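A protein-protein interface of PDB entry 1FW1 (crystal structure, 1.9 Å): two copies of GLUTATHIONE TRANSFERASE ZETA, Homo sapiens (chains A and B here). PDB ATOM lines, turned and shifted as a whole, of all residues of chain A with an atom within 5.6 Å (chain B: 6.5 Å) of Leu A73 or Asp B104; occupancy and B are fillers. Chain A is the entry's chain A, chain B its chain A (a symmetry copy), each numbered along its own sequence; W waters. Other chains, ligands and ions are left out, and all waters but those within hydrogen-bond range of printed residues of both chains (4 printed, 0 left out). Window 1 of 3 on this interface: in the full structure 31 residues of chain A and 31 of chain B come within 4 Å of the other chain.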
ATOM      1  N   ARG A  19      30.117  32.824 -18.975  1.00  0.00           N
ATOM      2  CA  ARG A  19      30.750  31.834 -19.889  1.00  0.00           C
ATOM      3  C   ARG A  19      31.621  32.533 -20.937  1.00  0.00           C
ATOM      4  O   ARG A  19      32.742  32.103 -21.203  1.00  0.00           O
ATOM      5  CB  ARG A  19      29.700  31.033 -20.666  1.00  0.00           C
ATOM      6  CG  ARG A  19      28.623  30.389 -19.793  1.00  0.00           C
ATOM      7  CD  ARG A  19      27.550  29.718 -20.721  1.00  0.00           C
ATOM      8  NE  ARG A  19      26.420  29.189 -19.974  1.00  0.00           N
ATOM      9  CZ  ARG A  19      25.175  29.179 -20.442  1.00  0.00           C
ATOM     10  NH1 ARG A  19      24.910  29.663 -21.647  1.00  0.00           N
ATOM     11  NH2 ARG A  19      24.192  28.697 -19.707  1.00  0.00           N
ATOM     12  N   GLN A  71      24.116  34.294 -28.541  1.00  0.00           N
ATOM     13  CA  GLN A  71      24.222  32.860 -28.130  1.00  0.00           C
ATOM     14  C   GLN A  71      25.622  32.543 -27.660  1.00  0.00           C
ATOM     15  O   GLN A  71      26.608  32.498 -28.457  1.00  0.00           O
ATOM     16  CB  GLN A  71      23.772  31.933 -29.253  1.00  0.00           C
ATOM     17  CG  GLN A  71      22.277  32.058 -29.552  1.00  0.00           C
ATOM     18  CD  GLN A  71      21.379  31.649 -28.382  1.00  0.00           C
ATOM     19  OE1 GLN A  71      21.762  30.848 -27.513  1.00  0.00           O
ATOM     20  NE2 GLN A  71      20.160  32.192 -28.360  1.00  0.00           N
ATOM     21  N   SER A  72      25.720  32.396 -26.342  1.00  0.00           N
ATOM     22  CA  SER A  72      27.001  32.196 -25.690  1.00  0.00           C
ATOM     23  C   SER A  72      27.866  31.121 -26.329  1.00  0.00           C
ATOM     24  O   SER A  72      29.026  31.361 -26.541  1.00  0.00           O
ATOM     25  CB  SER A  72      26.811  31.922 -24.185  1.00  0.00           C
ATOM     26  OG  SER A  72      26.083  30.727 -23.958  1.00  0.00           O
ATOM     27  N   LEU A  73      27.314  29.951 -26.659  1.00  0.00           N
ATOM     28  CA  LEU A  73      28.153  28.928 -27.258  1.00  0.00           C
ATOM     29  C   LEU A  73      28.526  29.261 -28.704  1.00  0.00           C
ATOM     30  O   LEU A  73      29.641  28.969 -29.127  1.00  0.00           O
ATOM     31  CB  LEU A  73      27.466  27.529 -27.160  1.00  0.00           C
ATOM     32  CG  LEU A  73      27.001  27.134 -25.747  1.00  0.00           C
ATOM     33  CD1 LEU A  73      26.460  25.637 -25.766  1.00  0.00           C
ATOM     34  CD2 LEU A  73      28.151  27.282 -24.732  1.00  0.00           C
ATOM     35  N   ALA A  74      27.624  29.842 -29.473  1.00  0.00           N
ATOM     36  CA  ALA A  74      27.982  30.202 -30.828  1.00  0.00           C
ATOM     37  C   ALA A  74      29.147  31.248 -30.789  1.00  0.00           C
ATOM     38  O   ALA A  74      30.032  31.258 -31.665  1.00  0.00           O
ATOM     39  CB  ALA A  74      26.800  30.801 -31.530  1.00  0.00           C
ATOM     40  N   ILE A  75      29.149  32.084 -29.754  1.00  0.00           N
ATOM     41  CA  ILE A  75      30.183  33.124 -29.592  1.00  0.00           C
ATOM     42  C   ILE A  75      31.465  32.413 -29.188  1.00  0.00           C
ATOM     43  O   ILE A  75      32.534  32.637 -29.747  1.00  0.00           O
ATOM     44  CB  ILE A  75      29.802  34.089 -28.446  1.00  0.00           C
ATOM     45  CG1 ILE A  75      28.644  34.991 -28.900  1.00  0.00           C
ATOM     46  CG2 ILE A  75      31.073  34.754 -27.908  1.00  0.00           C
ATOM     47  CD1 ILE A  75      27.997  35.791 -27.697  1.00  0.00           C
ATOM     48  N   ILE A  76      31.366  31.528 -28.211  1.00  0.00           N
ATOM     49  CA  ILE A  76      32.578  30.837 -27.812  1.00  0.00           C
ATOM     50  C   ILE A  76      33.152  30.029 -28.975  1.00  0.00           C
ATOM     51  O   ILE A  76      34.371  30.050 -29.183  1.00  0.00           O
ATOM     52  CB  ILE A  76      32.333  29.977 -26.547  1.00  0.00           C
ATOM     53  CG1 ILE A  76      32.023  30.919 -25.387  1.00  0.00           C
ATOM     54  CG2 ILE A  76      33.567  29.092 -26.208  1.00  0.00           C
ATOM     55  CD1 ILE A  76      31.462  30.207 -24.167  1.00  0.00           C
ATOM     56  N   GLU A  77      32.333  29.332 -29.760  1.00  0.00           N
ATOM     57  CA  GLU A  77      32.945  28.594 -30.882  1.00  0.00           C
ATOM     58  C   GLU A  77      33.518  29.552 -31.922  1.00  0.00           C
ATOM     59  O   GLU A  77      34.494  29.228 -32.611  1.00  0.00           O
ATOM     60  CB  GLU A  77      31.954  27.608 -31.540  1.00  0.00           C
ATOM     61  CG  GLU A  77      31.520  26.532 -30.529  1.00  0.00           C
ATOM     62  CD  GLU A  77      31.534  25.098 -31.110  1.00  0.00           C
ATOM     63  OE1 GLU A  77      32.378  24.790 -31.992  1.00  0.00           O
ATOM     64  OE2 GLU A  77      30.698  24.286 -30.662  1.00  0.00           O
ATOM     65  N   TYR A  78      32.929  30.732 -32.065  1.00  0.00           N
ATOM     66  CA  TYR A  78      33.493  31.692 -33.022  1.00  0.00           C
ATOM     67  C   TYR A  78      34.916  32.087 -32.581  1.00  0.00           C
ATOM     68  O   TYR A  78      35.838  32.166 -33.406  1.00  0.00           O
ATOM     69  CB  TYR A  78      32.622  32.929 -33.110  1.00  0.00           C
ATOM     70  CG  TYR A  78      33.210  33.946 -34.042  1.00  0.00           C
ATOM     71  CD1 TYR A  78      33.129  33.789 -35.432  1.00  0.00           C
ATOM     72  CD2 TYR A  78      33.894  35.064 -33.529  1.00  0.00           C
ATOM     73  CE1 TYR A  78      33.721  34.728 -36.290  1.00  0.00           C
ATOM     74  CE2 TYR A  78      34.498  36.011 -34.385  1.00  0.00           C
ATOM     75  CZ  TYR A  78      34.409  35.851 -35.732  1.00  0.00           C
ATOM     76  OH  TYR A  78      34.968  36.821 -36.540  1.00  0.00           O
ATOM     77  N   SER A 103      28.273  20.894 -22.619  1.00  0.00           N
ATOM     78  CA  SER A 103      27.940  22.301 -22.797  1.00  0.00           C
ATOM     79  C   SER A 103      26.432  22.477 -23.108  1.00  0.00           C
ATOM     80  O   SER A 103      25.771  23.303 -22.470  1.00  0.00           O
ATOM     81  CB  SER A 103      28.802  22.920 -23.917  1.00  0.00           C
ATOM     82  OG  SER A 103      30.176  22.841 -23.529  1.00  0.00           O
ATOM     83  N   ASP A 104      25.888  21.682 -24.040  1.00  0.00           N
ATOM     84  CA  ASP A 104      24.478  21.790 -24.397  1.00  0.00           C
ATOM     85  C   ASP A 104      23.571  21.358 -23.272  1.00  0.00           C
ATOM     86  O   ASP A 104      22.483  21.903 -23.105  1.00  0.00           O
ATOM     87  CB  ASP A 104      24.145  20.956 -25.647  1.00  0.00           C
ATOM     88  CG  ASP A 104      24.656  21.584 -26.913  1.00  0.00           C
ATOM     89  OD1 ASP A 104      25.290  22.685 -26.830  1.00  0.00           O
ATOM     90  OD2 ASP A 104      24.449  20.974 -27.994  1.00  0.00           O
ATOM     91  N   ALA A 107      23.757  24.548 -20.907  1.00  0.00           N
ATOM     92  CA  ALA A 107      23.216  25.756 -21.571  1.00  0.00           C
ATOM     93  C   ALA A 107      21.855  25.680 -22.220  1.00  0.00           C
ATOM     94  O   ALA A 107      21.170  26.725 -22.370  1.00  0.00           O
ATOM     95  CB  ALA A 107      24.217  26.287 -22.589  1.00  0.00           C
ATOM     96  N   MET A 161      35.350  24.211 -23.270  1.00  0.00           N
ATOM     97  CA  MET A 161      34.060  24.900 -23.247  1.00  0.00           C
ATOM     98  C   MET A 161      33.110  24.300 -22.213  1.00  0.00           C
ATOM     99  O   MET A 161      32.296  25.010 -21.610  1.00  0.00           O
ATOM    100  CB  MET A 161      33.412  24.858 -24.653  1.00  0.00           C
ATOM    101  CG  MET A 161      32.150  25.759 -24.808  1.00  0.00           C
ATOM    102  SD  MET A 161      31.602  25.881 -26.456  1.00  0.00           S
ATOM    103  CE  MET A 161      31.246  24.030 -26.791  1.00  0.00           C
ATOM    104  N   CYS A 165      30.989  26.371 -18.960  1.00  0.00           N
ATOM    105  CA  CYS A 165      29.568  26.307 -18.681  1.00  0.00           C
ATOM    106  C   CYS A 165      29.359  25.744 -17.276  1.00  0.00           C
ATOM    107  O   CYS A 165      28.415  26.133 -16.610  1.00  0.00           O
ATOM    108  CB  CYS A 165      28.790  25.401 -19.654  1.00  0.00           C
ATOM    109  SG  CYS A 165      28.802  25.874 -21.337  1.00  0.00           S
ATOM    110  N   LEU B  73      22.550  18.790 -31.075  1.00  0.00           N
ATOM    111  CA  LEU B  73      23.568  19.540 -31.790  1.00  0.00           C
ATOM    112  C   LEU B  73      24.965  18.947 -31.594  1.00  0.00           C
ATOM    113  O   LEU B  73      25.766  18.957 -32.526  1.00  0.00           O
ATOM    114  CB  LEU B  73      23.531  21.046 -31.376  1.00  0.00           C
ATOM    115  CG  LEU B  73      22.148  21.712 -31.482  1.00  0.00           C
ATOM    116  CD1 LEU B  73      22.285  23.269 -31.178  1.00  0.00           C
ATOM    117  CD2 LEU B  73      21.538  21.485 -32.879  1.00  0.00           C
ATOM    118  N   VAL B  99      25.039  30.203 -38.269  1.00  0.00           N
ATOM    119  CA  VAL B  99      24.415  28.863 -38.172  1.00  0.00           C
ATOM    120  C   VAL B  99      24.275  28.444 -36.720  1.00  0.00           C
ATOM    121  O   VAL B  99      23.195  28.023 -36.290  1.00  0.00           O
ATOM    122  CB  VAL B  99      25.252  27.774 -38.892  1.00  0.00           C
ATOM    123  CG1 VAL B  99      24.705  26.321 -38.546  1.00  0.00           C
ATOM    124  CG2 VAL B  99      25.201  28.026 -40.386  1.00  0.00           C
ATOM    125  N   ARG B 100      25.347  28.595 -35.945  1.00  0.00           N
ATOM    126  CA  ARG B 100      25.300  28.175 -34.559  1.00  0.00           C
ATOM    127  C   ARG B 100      24.363  29.005 -33.717  1.00  0.00           C
ATOM    128  O   ARG B 100      23.681  28.493 -32.824  1.00  0.00           O
ATOM    129  CB  ARG B 100      26.694  28.182 -33.931  1.00  0.00           C
ATOM    130  CG  ARG B 100      27.579  27.079 -34.434  1.00  0.00           C
ATOM    131  CD  ARG B 100      28.704  26.726 -33.419  1.00  0.00           C
ATOM    132  NE  ARG B 100      29.499  25.609 -33.914  1.00  0.00           N
ATOM    133  CZ  ARG B 100      30.581  25.724 -34.697  1.00  0.00           C
ATOM    134  NH1 ARG B 100      31.035  26.930 -35.070  1.00  0.00           N
ATOM    135  NH2 ARG B 100      31.182  24.623 -35.175  1.00  0.00           N
ATOM    136  N   MET B 101      24.334  30.307 -33.991  1.00  0.00           N
ATOM    137  CA  MET B 101      23.471  31.197 -33.246  1.00  0.00           C
ATOM    138  C   MET B 101      22.031  30.826 -33.517  1.00  0.00           C
ATOM    139  O   MET B 101      21.239  30.763 -32.600  1.00  0.00           O
ATOM    140  CB  MET B 101      23.721  32.680 -33.679  1.00  0.00           C
ATOM    141  CG  MET B 101      22.519  33.599 -33.426  1.00  0.00           C
ATOM    142  SD  MET B 101      22.978  35.384 -33.723  1.00  0.00           S
ATOM    143  CE  MET B 101      23.056  35.365 -35.548  1.00  0.00           C
ATOM    144  N   ILE B 102      21.666  30.627 -34.776  1.00  0.00           N
ATOM    145  CA  ILE B 102      20.275  30.285 -35.081  1.00  0.00           C
ATOM    146  C   ILE B 102      19.917  28.911 -34.471  1.00  0.00           C
ATOM    147  O   ILE B 102      18.815  28.753 -33.866  1.00  0.00           O
ATOM    148  CB  ILE B 102      20.008  30.292 -36.621  1.00  0.00           C
ATOM    149  CG1 ILE B 102      20.049  31.749 -37.162  1.00  0.00           C
ATOM    150  CG2 ILE B 102      18.618  29.757 -36.927  1.00  0.00           C
ATOM    151  CD1 ILE B 102      20.217  31.826 -38.704  1.00  0.00           C
ATOM    152  N   SER B 103      20.848  27.956 -34.590  1.00  0.00           N
ATOM    153  CA  SER B 103      20.637  26.630 -34.027  1.00  0.00           C
ATOM    154  C   SER B 103      20.417  26.708 -32.495  1.00  0.00           C
ATOM    155  O   SER B 103      19.456  26.121 -31.986  1.00  0.00           O
ATOM    156  CB  SER B 103      21.829  25.708 -34.359  1.00  0.00           C
ATOM    157  OG  SER B 103      21.915  25.572 -35.780  1.00  0.00           O
ATOM    158  N   ASP B 104      21.266  27.458 -31.778  1.00  0.00           N
ATOM    159  CA  ASP B 104      21.134  27.577 -30.331  1.00  0.00           C
ATOM    160  C   ASP B 104      19.886  28.326 -29.933  1.00  0.00           C
ATOM    161  O   ASP B 104      19.284  28.029 -28.904  1.00  0.00           O
ATOM    162  CB  ASP B 104      22.352  28.280 -29.707  1.00  0.00           C
ATOM    163  CG  ASP B 104      23.568  27.399 -29.662  1.00  0.00           C
ATOM    164  OD1 ASP B 104      23.477  26.217 -30.129  1.00  0.00           O
ATOM    165  OD2 ASP B 104      24.625  27.884 -29.182  1.00  0.00           O
ATOM    166  N   LEU B 105      19.492  29.313 -30.731  1.00  0.00           N
ATOM    167  CA  LEU B 105      18.272  30.057 -30.411  1.00  0.00           C
ATOM    168  C   LEU B 105      17.083  29.081 -30.398  1.00  0.00           C
ATOM    169  O   LEU B 105      16.271  29.069 -29.487  1.00  0.00           O
ATOM    170  CB  LEU B 105      18.018  31.153 -31.456  1.00  0.00           C
ATOM    171  CG  LEU B 105      16.818  32.088 -31.200  1.00  0.00           C
ATOM    172  CD1 LEU B 105      17.049  33.426 -31.959  1.00  0.00           C
ATOM    173  CD2 LEU B 105      15.543  31.450 -31.683  1.00  0.00           C
ATOM    174  N   ILE B 106      16.958  28.290 -31.441  1.00  0.00           N
ATOM    175  CA  ILE B 106      15.856  27.331 -31.502  1.00  0.00           C
ATOM    176  C   ILE B 106      16.019  26.246 -30.437  1.00  0.00           C
ATOM    177  O   ILE B 106      15.157  26.103 -29.548  1.00  0.00           O
ATOM    178  CB  ILE B 106      15.763  26.689 -32.936  1.00  0.00           C
ATOM    179  CG1 ILE B 106      15.322  27.746 -33.940  1.00  0.00           C
ATOM    180  CG2 ILE B 106      14.780  25.495 -32.986  1.00  0.00           C
ATOM    181  CD1 ILE B 106      15.639  27.392 -35.400  1.00  0.00           C
ATOM    182  N   ALA B 107      17.130  25.513 -30.480  1.00  0.00           N
ATOM    183  CA  ALA B 107      17.344  24.353 -29.584  1.00  0.00           C
ATOM    184  C   ALA B 107      17.534  24.602 -28.108  1.00  0.00           C
ATOM    185  O   ALA B 107      17.256  23.699 -27.277  1.00  0.00           O
ATOM    186  CB  ALA B 107      18.501  23.505 -30.093  1.00  0.00           C
ATOM    187  N   GLY B 108      18.008  25.812 -27.779  1.00  0.00           N
ATOM    188  CA  GLY B 108      18.237  26.157 -26.400  1.00  0.00           C
ATOM    189  C   GLY B 108      17.347  27.296 -25.902  1.00  0.00           C
ATOM    190  O   GLY B 108      17.145  27.438 -24.700  1.00  0.00           O
ATOM    191  N   GLY B 109      16.835  28.114 -26.819  1.00  0.00           N
ATOM    192  CA  GLY B 109      15.995  29.236 -26.417  1.00  0.00           C
ATOM    193  C   GLY B 109      14.500  29.153 -26.637  1.00  0.00           C
ATOM    194  O   GLY B 109      13.737  30.020 -26.121  1.00  0.00           O
ATOM    195  N   ILE B 110      14.055  28.138 -27.393  1.00  0.00           N
ATOM    196  CA  ILE B 110      12.631  27.950 -27.685  1.00  0.00           C
ATOM    197  C   ILE B 110      12.138  26.532 -27.302  1.00  0.00           C
ATOM    198  O   ILE B 110      11.279  26.371 -26.441  1.00  0.00           O
ATOM    199  CB  ILE B 110      12.318  28.156 -29.211  1.00  0.00           C
ATOM    200  CG1 ILE B 110      12.865  29.498 -29.710  1.00  0.00           C
ATOM    201  CG2 ILE B 110      10.782  28.162 -29.442  1.00  0.00           C
ATOM    202  CD1 ILE B 110      12.571  29.705 -31.218  1.00  0.00           C
ATOM    203  N   MET B 161      23.037  23.277 -40.490  1.00  0.00           N
ATOM    204  CA  MET B 161      22.477  22.859 -39.205  1.00  0.00           C
ATOM    205  C   MET B 161      21.333  23.768 -38.759  1.00  0.00           C
ATOM    206  O   MET B 161      20.379  23.318 -38.112  1.00  0.00           O
ATOM    207  CB  MET B 161      23.588  22.833 -38.127  1.00  0.00           C
ATOM    208  CG  MET B 161      23.161  22.181 -36.778  1.00  0.00           C
ATOM    209  SD  MET B 161      24.496  21.943 -35.687  1.00  0.00           S
ATOM    210  CE  MET B 161      25.054  23.765 -35.494  1.00  0.00           C
ATOM    211  N   CYS B 165      17.242  22.610 -37.621  1.00  0.00           N
ATOM    212  CA  CYS B 165      16.548  22.985 -36.404  1.00  0.00           C
ATOM    213  C   CYS B 165      15.286  23.764 -36.768  1.00  0.00           C
ATOM    214  O   CYS B 165      14.295  23.661 -36.066  1.00  0.00           O
ATOM    215  CB  CYS B 165      17.383  23.883 -35.471  1.00  0.00           C
ATOM    216  SG  CYS B 165      18.859  23.191 -34.840  1.00  0.00           S
HETATM  217  O   HOH W   1      26.805  26.923 -30.553  1.00  0.00           O
HETATM  218  O   HOH W   2      21.829  19.896 -28.416  1.00  0.00           O
HETATM  219  O   HOH W   3      30.198  29.656 -34.090  1.00  0.00           O
HETATM  220  O   HOH W   4      24.402  29.380 -26.750  1.00  0.00           O
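OE1 of Glu A77 is in salt-bridge range of NH2 of Arg B100.
The backbone NH (N) of Ile B110 is in hydrogen-bond range of the backbone carbonyl oxygen (O) of Leu B105, 3.2 Å away. O of Asp B104 sits at hydrogen-bond distance from N of Gly B109 (3.2 Å).
Gln A71 touches Met B101. Gln A71 touches Asp B104 (OE1 to CB, 3.4 Å). Gln A71 touches Leu B105. Leu A73 touches Asp B104 (CB to OD2, 3.5 Å). Arg B100 touches Ala A74. CB of Ala A74 touches N of Met B101 (3.5 Å). Asp B104 touches Ala A74 (OD2 to N, 3.6 Å). Leu B73 touches Asp A104 (CB to OD2, 3.5 Å).
Leu A73 touches just one residue of chain B: Asp B104. Of the printed residues of chain A, Met B101 touches Gln A71 and Ala A74. Printed residues of chain B within 4 Å of Ala A74: Arg B100, Met B101 and Asp B104. Of the printed residues of chain B, Asp A104 touches Leu B73 (3.5 Å). Of the printed residues of chain A, Leu B105 touches Gln A71 (3.5 Å). Ser A103 touches none of the printed residues of chain B. The nearest printed residue of chain A that does not touch Met B101 is Ile A75 (6.7 Å).
Printed residues of chain B that touch a printed residue of chain A: Leu B73, Arg B100, Met B101, Asp B104 and Leu B105. Hydrophobic or aromatic side chains of chain B within 4 Å of the printed part of chain A: Leu B73 and Leu B105. Hydrophobic or aromatic side chains of chain A that line the printed part of chain B: Leu A73 and Ala A74. Among the printed residues, Asp or Glu carboxylates within 4 Å of a Lys or Arg side-chain nitrogen of the other chain: Glu A77 with Arg B100 (3.4 Å).
Leu A73 touches Asp B104, and with the chains exchanged Asp A104 touches Leu B73. Positions printed for both chains: 73, 103, 104, 107, 161 and 165. Of the 9 pairs that touch across the chains among the printed residues, 2 have their exchanged pair printed and touching as well.
Water W1 bridges the side-chain carboxylate of Asp B104 and the backbone NH of Ala A74. Water W2 lies within hydrogen-bond range of the side-chain carboxylate of Asp A104 (2.9 Å) and the backbone NH of Leu B73 (3.0 Å). Water W4 lies within hydrogen-bond range of the side-chain carboxylate of Asp B104 (2.9 Å), the backbone NH of Leu A73 (3.0 Å), the side-chain amide oxygen of Gln A71 (3.1 Å) and the backbone NH of Ser A72 (3.3 Å). Water W3 bridges the backbone carbonyl oxygen (O) of Ala A74 (2.9 Å) and the guanidinium group (NH1) of Arg B100 (3.0 Å).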
